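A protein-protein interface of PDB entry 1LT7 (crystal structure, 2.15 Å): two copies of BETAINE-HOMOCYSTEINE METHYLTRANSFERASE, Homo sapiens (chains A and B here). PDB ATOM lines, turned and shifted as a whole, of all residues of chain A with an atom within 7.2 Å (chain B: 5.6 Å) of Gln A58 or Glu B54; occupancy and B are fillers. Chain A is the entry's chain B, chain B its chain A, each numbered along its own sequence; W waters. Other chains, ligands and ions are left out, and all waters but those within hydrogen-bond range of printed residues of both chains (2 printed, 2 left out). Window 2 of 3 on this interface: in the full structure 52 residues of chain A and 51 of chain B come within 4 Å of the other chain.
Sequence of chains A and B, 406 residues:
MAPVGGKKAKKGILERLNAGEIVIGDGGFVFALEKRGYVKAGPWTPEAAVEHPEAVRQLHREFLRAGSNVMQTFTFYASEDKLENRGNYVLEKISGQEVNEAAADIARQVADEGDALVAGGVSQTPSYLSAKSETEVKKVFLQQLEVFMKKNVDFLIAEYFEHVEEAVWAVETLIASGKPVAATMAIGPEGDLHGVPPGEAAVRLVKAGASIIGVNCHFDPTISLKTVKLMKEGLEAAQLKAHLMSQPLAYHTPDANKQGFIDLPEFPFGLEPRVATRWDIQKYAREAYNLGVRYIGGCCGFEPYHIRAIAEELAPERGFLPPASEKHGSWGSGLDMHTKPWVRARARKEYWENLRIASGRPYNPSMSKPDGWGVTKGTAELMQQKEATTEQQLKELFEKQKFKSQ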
ATOM      1  N   PHE A  29      29.888  -3.863 -25.328  1.00  0.00           N
ATOM      2  CA  PHE A  29      28.484  -3.919 -24.933  1.00  0.00           C
ATOM      3  C   PHE A  29      28.276  -5.251 -24.259  1.00  0.00           C
ATOM      4  O   PHE A  29      27.834  -5.325 -23.119  1.00  0.00           O
ATOM      5  CB  PHE A  29      27.543  -3.824 -26.133  1.00  0.00           C
ATOM      6  CG  PHE A  29      26.090  -3.922 -25.751  1.00  0.00           C
ATOM      7  CD1 PHE A  29      25.349  -2.775 -25.484  1.00  0.00           C
ATOM      8  CD2 PHE A  29      25.483  -5.171 -25.576  1.00  0.00           C
ATOM      9  CE1 PHE A  29      24.032  -2.859 -25.044  1.00  0.00           C
ATOM     10  CE2 PHE A  29      24.143  -5.279 -25.127  1.00  0.00           C
ATOM     11  CZ  PHE A  29      23.418  -4.117 -24.862  1.00  0.00           C
ATOM     12  N   ARG A  36      27.365  -6.519 -15.630  1.00  0.00           N
ATOM     13  CA  ARG A  36      26.225  -6.031 -14.854  1.00  0.00           C
ATOM     14  C   ARG A  36      25.258  -7.151 -14.426  1.00  0.00           C
ATOM     15  O   ARG A  36      24.299  -6.896 -13.710  1.00  0.00           O
ATOM     16  CB  ARG A  36      25.493  -4.934 -15.637  1.00  0.00           C
ATOM     17  CG  ARG A  36      26.433  -3.851 -16.131  1.00  0.00           C
ATOM     18  CD  ARG A  36      25.739  -2.601 -16.547  1.00  0.00           C
ATOM     19  NE  ARG A  36      26.711  -1.583 -16.917  1.00  0.00           N
ATOM     20  CZ  ARG A  36      26.401  -0.355 -17.330  1.00  0.00           C
ATOM     21  NH1 ARG A  36      25.135   0.025 -17.426  1.00  0.00           N
ATOM     22  NH2 ARG A  36      27.363   0.499 -17.637  1.00  0.00           N
ATOM     23  N   PRO A  53      14.581  -5.603 -20.393  1.00  0.00           N
ATOM     24  CA  PRO A  53      14.839  -4.705 -21.525  1.00  0.00           C
ATOM     25  C   PRO A  53      15.420  -3.388 -21.017  1.00  0.00           C
ATOM     26  O   PRO A  53      16.275  -2.778 -21.652  1.00  0.00           O
ATOM     27  CB  PRO A  53      13.454  -4.513 -22.139  1.00  0.00           C
ATOM     28  CG  PRO A  53      12.710  -5.730 -21.697  1.00  0.00           C
ATOM     29  CD  PRO A  53      13.153  -5.926 -20.300  1.00  0.00           C
ATOM     30  N   GLU A  54      14.936  -2.965 -19.858  1.00  0.00           N
ATOM     31  CA  GLU A  54      15.394  -1.743 -19.241  1.00  0.00           C
ATOM     32  C   GLU A  54      16.912  -1.747 -19.015  1.00  0.00           C
ATOM     33  O   GLU A  54      17.567  -0.719 -19.211  1.00  0.00           O
ATOM     34  CB  GLU A  54      14.656  -1.513 -17.913  1.00  0.00           C
ATOM     35  CG  GLU A  54      13.827  -2.699 -17.404  1.00  0.00           C
ATOM     36  CD  GLU A  54      14.672  -3.808 -16.835  1.00  0.00           C
ATOM     37  OE1 GLU A  54      15.526  -4.315 -17.563  1.00  0.00           O
ATOM     38  OE2 GLU A  54      14.492  -4.182 -15.657  1.00  0.00           O
ATOM     39  N   ALA A  55      17.464  -2.903 -18.648  1.00  0.00           N
ATOM     40  CA  ALA A  55      18.890  -3.005 -18.388  1.00  0.00           C
ATOM     41  C   ALA A  55      19.665  -2.865 -19.676  1.00  0.00           C
ATOM     42  O   ALA A  55      20.717  -2.221 -19.715  1.00  0.00           O
ATOM     43  CB  ALA A  55      19.233  -4.328 -17.732  1.00  0.00           C
ATOM     44  N   VAL A  56      19.138  -3.473 -20.735  1.00  0.00           N
ATOM     45  CA  VAL A  56      19.785  -3.422 -22.032  1.00  0.00           C
ATOM     46  C   VAL A  56      19.639  -2.027 -22.656  1.00  0.00           C
ATOM     47  O   VAL A  56      20.582  -1.498 -23.226  1.00  0.00           O
ATOM     48  CB  VAL A  56      19.196  -4.524 -22.958  1.00  0.00           C
ATOM     49  CG1 VAL A  56      19.816  -4.454 -24.344  1.00  0.00           C
ATOM     50  CG2 VAL A  56      19.456  -5.910 -22.334  1.00  0.00           C
ATOM     51  N   ARG A  57      18.468  -1.414 -22.539  1.00  0.00           N
ATOM     52  CA  ARG A  57      18.269  -0.084 -23.103  1.00  0.00           C
ATOM     53  C   ARG A  57      19.175   0.956 -22.433  1.00  0.00           C
ATOM     54  O   ARG A  57      19.713   1.840 -23.086  1.00  0.00           O
ATOM     55  CB  ARG A  57      16.796   0.348 -22.954  1.00  0.00           C
ATOM     56  CG  ARG A  57      16.543   1.839 -23.201  1.00  0.00           C
ATOM     57  CD  ARG A  57      15.049   2.168 -23.198  1.00  0.00           C
ATOM     58  NE  ARG A  57      14.365   1.374 -24.218  1.00  0.00           N
ATOM     59  CZ  ARG A  57      13.552   0.356 -23.960  1.00  0.00           C
ATOM     60  NH1 ARG A  57      12.979  -0.314 -24.956  1.00  0.00           N
ATOM     61  NH2 ARG A  57      13.285   0.028 -22.702  1.00  0.00           N
ATOM     62  N   GLN A  58      19.302   0.856 -21.121  1.00  0.00           N
ATOM     63  CA  GLN A  58      20.138   1.761 -20.331  1.00  0.00           C
ATOM     64  C   GLN A  58      21.629   1.674 -20.736  1.00  0.00           C
ATOM     65  O   GLN A  58      22.309   2.689 -20.850  1.00  0.00           O
ATOM     66  CB  GLN A  58      19.950   1.423 -18.841  1.00  0.00           C
ATOM     67  CG  GLN A  58      20.700   2.289 -17.845  1.00  0.00           C
ATOM     68  CD  GLN A  58      20.586   3.765 -18.146  1.00  0.00           C
ATOM     69  OE1 GLN A  58      19.496   4.266 -18.457  1.00  0.00           O
ATOM     70  NE2 GLN A  58      21.712   4.482 -18.040  1.00  0.00           N
ATOM     71  N   LEU A  59      22.124   0.464 -20.970  1.00  0.00           N
ATOM     72  CA  LEU A  59      23.516   0.280 -21.355  1.00  0.00           C
ATOM     73  C   LEU A  59      23.760   0.891 -22.719  1.00  0.00           C
ATOM     74  O   LEU A  59      24.733   1.625 -22.899  1.00  0.00           O
ATOM     75  CB  LEU A  59      23.883  -1.207 -21.370  1.00  0.00           C
ATOM     76  CG  LEU A  59      25.332  -1.575 -21.767  1.00  0.00           C
ATOM     77  CD1 LEU A  59      26.372  -0.674 -21.008  1.00  0.00           C
ATOM     78  CD2 LEU A  59      25.539  -3.046 -21.491  1.00  0.00           C
ATOM     79  N   HIS A  60      22.869   0.598 -23.676  1.00  0.00           N
ATOM     80  CA  HIS A  60      22.970   1.155 -25.031  1.00  0.00           C
ATOM     81  C   HIS A  60      23.030   2.681 -24.922  1.00  0.00           C
ATOM     82  O   HIS A  60      23.845   3.326 -25.579  1.00  0.00           O
ATOM     83  CB  HIS A  60      21.742   0.763 -25.886  1.00  0.00           C
ATOM     84  CG  HIS A  60      21.853  -0.574 -26.545  1.00  0.00           C
ATOM     85  ND1 HIS A  60      22.910  -0.912 -27.364  1.00  0.00           N
ATOM     86  CD2 HIS A  60      21.030  -1.654 -26.529  1.00  0.00           C
ATOM     87  CE1 HIS A  60      22.741  -2.143 -27.821  1.00  0.00           C
ATOM     88  NE2 HIS A  60      21.609  -2.618 -27.328  1.00  0.00           N
ATOM     89  N   ARG A  61      22.166   3.252 -24.093  1.00  0.00           N
ATOM     90  CA  ARG A  61      22.115   4.704 -23.900  1.00  0.00           C
ATOM     91  C   ARG A  61      23.413   5.282 -23.328  1.00  0.00           C
ATOM     92  O   ARG A  61      23.847   6.382 -23.713  1.00  0.00           O
ATOM     93  CB  ARG A  61      20.941   5.060 -22.988  1.00  0.00           C
ATOM     94  CG  ARG A  61      19.596   5.017 -23.725  1.00  0.00           C
ATOM     95  CD  ARG A  61      18.427   5.385 -22.832  1.00  0.00           C
ATOM     96  NE  ARG A  61      17.185   5.511 -23.599  1.00  0.00           N
ATOM     97  CZ  ARG A  61      15.976   5.352 -23.069  1.00  0.00           C
ATOM     98  NH1 ARG A  61      14.888   5.487 -23.814  1.00  0.00           N
ATOM     99  NH2 ARG A  61      15.859   5.045 -21.781  1.00  0.00           N
ATOM    100  N   GLU A  62      24.035   4.537 -22.413  1.00  0.00           N
ATOM    101  CA  GLU A  62      25.285   5.003 -21.835  1.00  0.00           C
ATOM    102  C   GLU A  62      26.320   5.041 -22.939  1.00  0.00           C
ATOM    103  O   GLU A  62      27.048   6.012 -23.061  1.00  0.00           O
ATOM    104  CB  GLU A  62      25.700   4.104 -20.665  1.00  0.00           C
ATOM    105  CG  GLU A  62      24.814   4.367 -19.424  1.00  0.00           C
ATOM    106  CD  GLU A  62      25.128   3.427 -18.287  1.00  0.00           C
ATOM    107  OE1 GLU A  62      26.305   2.990 -18.195  1.00  0.00           O
ATOM    108  OE2 GLU A  62      24.212   3.129 -17.494  1.00  0.00           O
ATOM    109  N   PHE A  63      26.378   4.012 -23.778  1.00  0.00           N
ATOM    110  CA  PHE A  63      27.332   4.094 -24.864  1.00  0.00           C
ATOM    111  C   PHE A  63      27.046   5.291 -25.788  1.00  0.00           C
ATOM    112  O   PHE A  63      27.968   6.014 -26.180  1.00  0.00           O
ATOM    113  CB  PHE A  63      27.337   2.820 -25.667  1.00  0.00           C
ATOM    114  CG  PHE A  63      28.161   1.711 -25.038  1.00  0.00           C
ATOM    115  CD1 PHE A  63      27.544   0.590 -24.486  1.00  0.00           C
ATOM    116  CD2 PHE A  63      29.552   1.830 -24.936  1.00  0.00           C
ATOM    117  CE1 PHE A  63      28.307  -0.393 -23.828  1.00  0.00           C
ATOM    118  CE2 PHE A  63      30.314   0.844 -24.281  1.00  0.00           C
ATOM    119  CZ  PHE A  63      29.692  -0.255 -23.731  1.00  0.00           C
ATOM    120  N   LEU A  64      25.773   5.507 -26.134  1.00  0.00           N
ATOM    121  CA  LEU A  64      25.401   6.617 -27.008  1.00  0.00           C
ATOM    122  C   LEU A  64      25.769   7.949 -26.356  1.00  0.00           C
ATOM    123  O   LEU A  64      26.273   8.844 -26.992  1.00  0.00           O
ATOM    124  CB  LEU A  64      23.886   6.623 -27.289  1.00  0.00           C
ATOM    125  CG  LEU A  64      23.454   7.682 -28.335  1.00  0.00           C
ATOM    126  CD1 LEU A  64      23.691   7.111 -29.734  1.00  0.00           C
ATOM    127  CD2 LEU A  64      21.976   8.067 -28.156  1.00  0.00           C
ATOM    128  N   ARG A  65      25.486   8.071 -25.072  1.00  0.00           N
ATOM    129  CA  ARG A  65      25.764   9.299 -24.354  1.00  0.00           C
ATOM    130  C   ARG A  65      27.283   9.517 -24.341  1.00  0.00           C
ATOM    131  O   ARG A  65      27.739  10.662 -24.389  1.00  0.00           O
ATOM    132  CB  ARG A  65      25.161   9.171 -22.943  1.00  0.00           C
ATOM    133  CG  ARG A  65      25.553  10.213 -21.905  1.00  0.00           C
ATOM    134  CD  ARG A  65      24.756   9.971 -20.597  1.00  0.00           C
ATOM    135  NE  ARG A  65      24.849  11.123 -19.713  1.00  0.00           N
ATOM    136  CZ  ARG A  65      24.188  12.260 -19.923  1.00  0.00           C
ATOM    137  NH1 ARG A  65      23.383  12.379 -20.972  1.00  0.00           N
ATOM    138  NH2 ARG A  65      24.358  13.294 -19.113  1.00  0.00           N
ATOM    139  N   ILE A 106      15.435  -2.761 -29.368  1.00  0.00           N
ATOM    140  CA  ILE A 106      15.990  -1.886 -28.341  1.00  0.00           C
ATOM    141  C   ILE A 106      17.181  -1.114 -28.906  1.00  0.00           C
ATOM    142  O   ILE A 106      17.300   0.097 -28.709  1.00  0.00           O
ATOM    143  CB  ILE A 106      16.382  -2.720 -27.089  1.00  0.00           C
ATOM    144  CG1 ILE A 106      15.107  -3.237 -26.419  1.00  0.00           C
ATOM    145  CG2 ILE A 106      17.133  -1.862 -26.077  1.00  0.00           C
ATOM    146  CD1 ILE A 106      15.374  -4.108 -25.240  1.00  0.00           C
ATOM    147  N   VAL A 110      17.346   3.010 -29.274  1.00  0.00           N
ATOM    148  CA  VAL A 110      18.324   3.943 -28.708  1.00  0.00           C
ATOM    149  C   VAL A 110      19.125   4.630 -29.788  1.00  0.00           C
ATOM    150  O   VAL A 110      19.527   5.781 -29.637  1.00  0.00           O
ATOM    151  CB  VAL A 110      19.273   3.219 -27.717  1.00  0.00           C
ATOM    152  CG1 VAL A 110      20.359   4.188 -27.202  1.00  0.00           C
ATOM    153  CG2 VAL A 110      18.456   2.659 -26.564  1.00  0.00           C
ATOM    154  N   PRO A 304      31.454   2.254 -21.009  1.00  0.00           N
ATOM    155  CA  PRO A 304      31.102   3.572 -21.530  1.00  0.00           C
ATOM    156  C   PRO A 304      32.170   4.641 -21.296  1.00  0.00           C
ATOM    157  O   PRO A 304      32.445   5.420 -22.207  1.00  0.00           O
ATOM    158  CB  PRO A 304      29.754   3.873 -20.827  1.00  0.00           C
ATOM    159  CG  PRO A 304      29.103   2.484 -20.890  1.00  0.00           C
ATOM    160  CD  PRO A 304      30.282   1.624 -20.374  1.00  0.00           C
ATOM    161  N   TYR B  38      26.789  10.232 -14.550  1.00  0.00           N
ATOM    162  CA  TYR B  38      25.601  11.007 -14.243  1.00  0.00           C
ATOM    163  C   TYR B  38      25.863  11.795 -12.973  1.00  0.00           C
ATOM    164  O   TYR B  38      24.906  12.004 -12.210  1.00  0.00           O
ATOM    165  CB  TYR B  38      24.399  10.067 -14.055  1.00  0.00           C
ATOM    166  CG  TYR B  38      24.026   9.290 -15.294  1.00  0.00           C
ATOM    167  CD1 TYR B  38      23.219   9.853 -16.274  1.00  0.00           C
ATOM    168  CD2 TYR B  38      24.483   7.988 -15.490  1.00  0.00           C
ATOM    169  CE1 TYR B  38      22.865   9.133 -17.432  1.00  0.00           C
ATOM    170  CE2 TYR B  38      24.146   7.268 -16.633  1.00  0.00           C
ATOM    171  CZ  TYR B  38      23.338   7.847 -17.599  1.00  0.00           C
ATOM    172  OH  TYR B  38      23.017   7.144 -18.732  1.00  0.00           O
ATOM    173  N   HIS B  52      18.537  11.773 -14.899  1.00  0.00           N
ATOM    174  CA  HIS B  52      18.089  10.562 -15.633  1.00  0.00           C
ATOM    175  C   HIS B  52      17.691   9.564 -14.585  1.00  0.00           C
ATOM    176  O   HIS B  52      18.479   8.708 -14.204  1.00  0.00           O
ATOM    177  CB  HIS B  52      19.226  10.011 -16.477  1.00  0.00           C
ATOM    178  CG  HIS B  52      19.711  10.975 -17.507  1.00  0.00           C
ATOM    179  ND1 HIS B  52      19.238  10.988 -18.803  1.00  0.00           N
ATOM    180  CD2 HIS B  52      20.568  12.017 -17.412  1.00  0.00           C
ATOM    181  CE1 HIS B  52      19.786  11.998 -19.459  1.00  0.00           C
ATOM    182  NE2 HIS B  52      20.598  12.637 -18.634  1.00  0.00           N
ATOM    183  N   PRO B  53      16.462   9.703 -14.067  1.00  0.00           N
ATOM    184  CA  PRO B  53      15.941   8.803 -13.044  1.00  0.00           C
ATOM    185  C   PRO B  53      16.031   7.341 -13.465  1.00  0.00           C
ATOM    186  O   PRO B  53      16.182   6.463 -12.629  1.00  0.00           O
ATOM    187  CB  PRO B  53      14.486   9.282 -12.859  1.00  0.00           C
ATOM    188  CG  PRO B  53      14.163   9.973 -14.186  1.00  0.00           C
ATOM    189  CD  PRO B  53      15.457  10.716 -14.442  1.00  0.00           C
ATOM    190  N   GLU B  54      15.941   7.077 -14.761  1.00  0.00           N
ATOM    191  CA  GLU B  54      16.009   5.702 -15.211  1.00  0.00           C
ATOM    192  C   GLU B  54      17.426   5.168 -15.004  1.00  0.00           C
ATOM    193  O   GLU B  54      17.582   4.018 -14.609  1.00  0.00           O
ATOM    194  CB  GLU B  54      15.570   5.562 -16.681  1.00  0.00           C
ATOM    195  CG  GLU B  54      16.474   6.224 -17.714  1.00  0.00           C
ATOM    196  CD  GLU B  54      16.345   7.753 -17.786  1.00  0.00           C
ATOM    197  OE1 GLU B  54      16.980   8.348 -18.671  1.00  0.00           O
ATOM    198  OE2 GLU B  54      15.629   8.360 -16.972  1.00  0.00           O
ATOM    199  N   ALA B  55      18.436   6.005 -15.269  1.00  0.00           N
ATOM    200  CA  ALA B  55      19.822   5.627 -15.061  1.00  0.00           C
ATOM    201  C   ALA B  55      20.043   5.319 -13.580  1.00  0.00           C
ATOM    202  O   ALA B  55      20.745   4.349 -13.233  1.00  0.00           O
ATOM    203  CB  ALA B  55      20.764   6.749 -15.491  1.00  0.00           C
ATOM    204  N   VAL B  56      19.459   6.139 -12.712  1.00  0.00           N
ATOM    205  CA  VAL B  56      19.589   5.953 -11.272  1.00  0.00           C
ATOM    206  C   VAL B  56      18.814   4.722 -10.824  1.00  0.00           C
ATOM    207  O   VAL B  56      19.287   3.943  -9.999  1.00  0.00           O
ATOM    208  CB  VAL B  56      19.079   7.193 -10.508  1.00  0.00           C
ATOM    209  CG1 VAL B  56      18.964   6.917  -9.022  1.00  0.00           C
ATOM    210  CG2 VAL B  56      20.039   8.326 -10.724  1.00  0.00           C
ATOM    211  N   ARG B  57      17.619   4.535 -11.381  1.00  0.00           N
ATOM    212  CA  ARG B  57      16.819   3.377 -11.022  1.00  0.00           C
ATOM    213  C   ARG B  57      17.520   2.070 -11.435  1.00  0.00           C
ATOM    214  O   ARG B  57      17.527   1.110 -10.681  1.00  0.00           O
ATOM    215  CB  ARG B  57      15.430   3.447 -11.679  1.00  0.00           C
ATOM    216  CG  ARG B  57      14.587   2.185 -11.461  1.00  0.00           C
ATOM    217  CD  ARG B  57      13.219   2.298 -12.128  1.00  0.00           C
ATOM    218  NE  ARG B  57      12.394   3.356 -11.543  1.00  0.00           N
ATOM    219  CZ  ARG B  57      12.272   4.595 -12.014  1.00  0.00           C
ATOM    220  NH1 ARG B  57      11.481   5.464 -11.378  1.00  0.00           N
ATOM    221  NH2 ARG B  57      12.910   4.974 -13.124  1.00  0.00           N
ATOM    222  N   GLN B  58      18.081   2.024 -12.638  1.00  0.00           N
ATOM    223  CA  GLN B  58      18.787   0.820 -13.090  1.00  0.00           C
ATOM    224  C   GLN B  58      19.971   0.475 -12.148  1.00  0.00           C
ATOM    225  O   GLN B  58      20.090  -0.649 -11.694  1.00  0.00           O
ATOM    226  CB  GLN B  58      19.286   1.002 -14.534  1.00  0.00           C
ATOM    227  CG  GLN B  58      20.212  -0.117 -15.056  1.00  0.00           C
ATOM    228  CD  GLN B  58      19.566  -1.511 -15.096  1.00  0.00           C
ATOM    229  OE1 GLN B  58      20.270  -2.544 -15.081  1.00  0.00           O
ATOM    230  NE2 GLN B  58      18.224  -1.549 -15.165  1.00  0.00           N
ATOM    231  N   LEU B  59      20.826   1.451 -11.835  1.00  0.00           N
ATOM    232  CA  LEU B  59      21.955   1.203 -10.968  1.00  0.00           C
ATOM    233  C   LEU B  59      21.455   0.599  -9.672  1.00  0.00           C
ATOM    234  O   LEU B  59      22.035  -0.376  -9.196  1.00  0.00           O
ATOM    235  CB  LEU B  59      22.745   2.497 -10.690  1.00  0.00           C
ATOM    236  CG  LEU B  59      23.948   2.368  -9.735  1.00  0.00           C
ATOM    237  CD1 LEU B  59      24.873   1.200 -10.147  1.00  0.00           C
ATOM    238  CD2 LEU B  59      24.709   3.682  -9.732  1.00  0.00           C
ATOM    239  N   ILE B 106      12.998   7.020  -5.943  1.00  0.00           N
ATOM    240  CA  ILE B 106      13.551   5.946  -6.792  1.00  0.00           C
ATOM    241  C   ILE B 106      14.147   4.855  -5.888  1.00  0.00           C
ATOM    242  O   ILE B 106      13.842   3.674  -6.052  1.00  0.00           O
ATOM    243  CB  ILE B 106      14.669   6.462  -7.766  1.00  0.00           C
ATOM    244  CG1 ILE B 106      14.118   7.549  -8.695  1.00  0.00           C
ATOM    245  CG2 ILE B 106      15.132   5.345  -8.670  1.00  0.00           C
ATOM    246  CD1 ILE B 106      15.167   8.105  -9.640  1.00  0.00           C
HETATM  247  O   HOH W   1      22.836   2.966 -14.838  1.00  0.00           O
HETATM  248  O   HOH W   2      22.507  -1.581 -17.541  1.00  0.00           O
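The side-chain carboxylate (OE2) of Glu A62 lies within hydrogen-bond range of the side-chain amide nitrogen (NE2) of Gln A58 (2.9 Å).
ND1 of His B52 is in hydrogen-bond range of OE1 of Glu B54 (3.5 Å).
The guanidinium group of Arg A36 is in salt-bridge range of the side-chain carboxylate of Glu A62, at 2.8 Å.
The side-chain hydroxyl of Tyr B38 lies within hydrogen-bond range of the side-chain amide nitrogen of Gln A58, at 3.0 Å.
Water W2 lies within hydrogen-bond range of O of Ala A55 (2.9 Å), NH1 of Arg A36 (3.1 Å) and OE1 of Gln B58 (3.5 Å).
Water W1 bridges O of Ala B55 and OE2 of Glu A62.
Ala A55 touches Gln B58 (CB to OE1, 3.4 Å).
Glu B54 touches Gln A58 (CG to OE1, 3.7 Å).
Gln A58 touches Ala B55 (NE2 to CB, 3.5 Å).
Gln A58 touches Gln B58.
Tyr B38 touches Glu A62.
NE of Arg A65 touches CE1 of Tyr B38 (3.6 Å).
NH1 of Arg A65 touches NE2 of His B52, at 3.6 Å.
Of chain B, only Tyr B38, Glu B54, Ala B55 and Gln B58 come within 4 Å of Gln A58.
Glu B54 touches just one residue of chain A: Gln A58.
Printed residues of chain B within 4 Å of Arg A65: Tyr B38 (3.6 Å) and His B52 (3.6 Å).
Of the printed residues of chain B, Ala A55 touches Gln B58.
Val A56 touches none of the printed residues of chain B.
Phe A63 touches none of the printed residues of chain B.
The nearest printed residue of chain B that does not touch Gln A58 is Val B56 (6.0 Å).
The nearest residue of chain A that does not touch Glu B54 is Arg A61 (4.3 Å).
The nearest printed residue of chain A that does not touch Tyr B38 is Arg A61 (5.0 Å).
Ala A55 touches Gln B58, and with the chains exchanged Gln A58 touches Ala B55.
Gln A58 touches Glu B54, but with the chains exchanged Glu A54 does not touch Gln B58 (4.1 Å).
Gln A58 touches its own counterpart, Gln B58.
Hydrophobic or aromatic side chains of chain B that line the printed part of chain A: Tyr B38, His B52 and Ala B55.
Printed residues of chain A that touch a printed residue of chain B: Ala A55, Gln A58, Glu A62 and Arg A65.
Hydrophobic or aromatic side chains of chain A that line the printed part of chain B: Ala A55.
Among the printed residues, 8 pairs touch across the chains.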
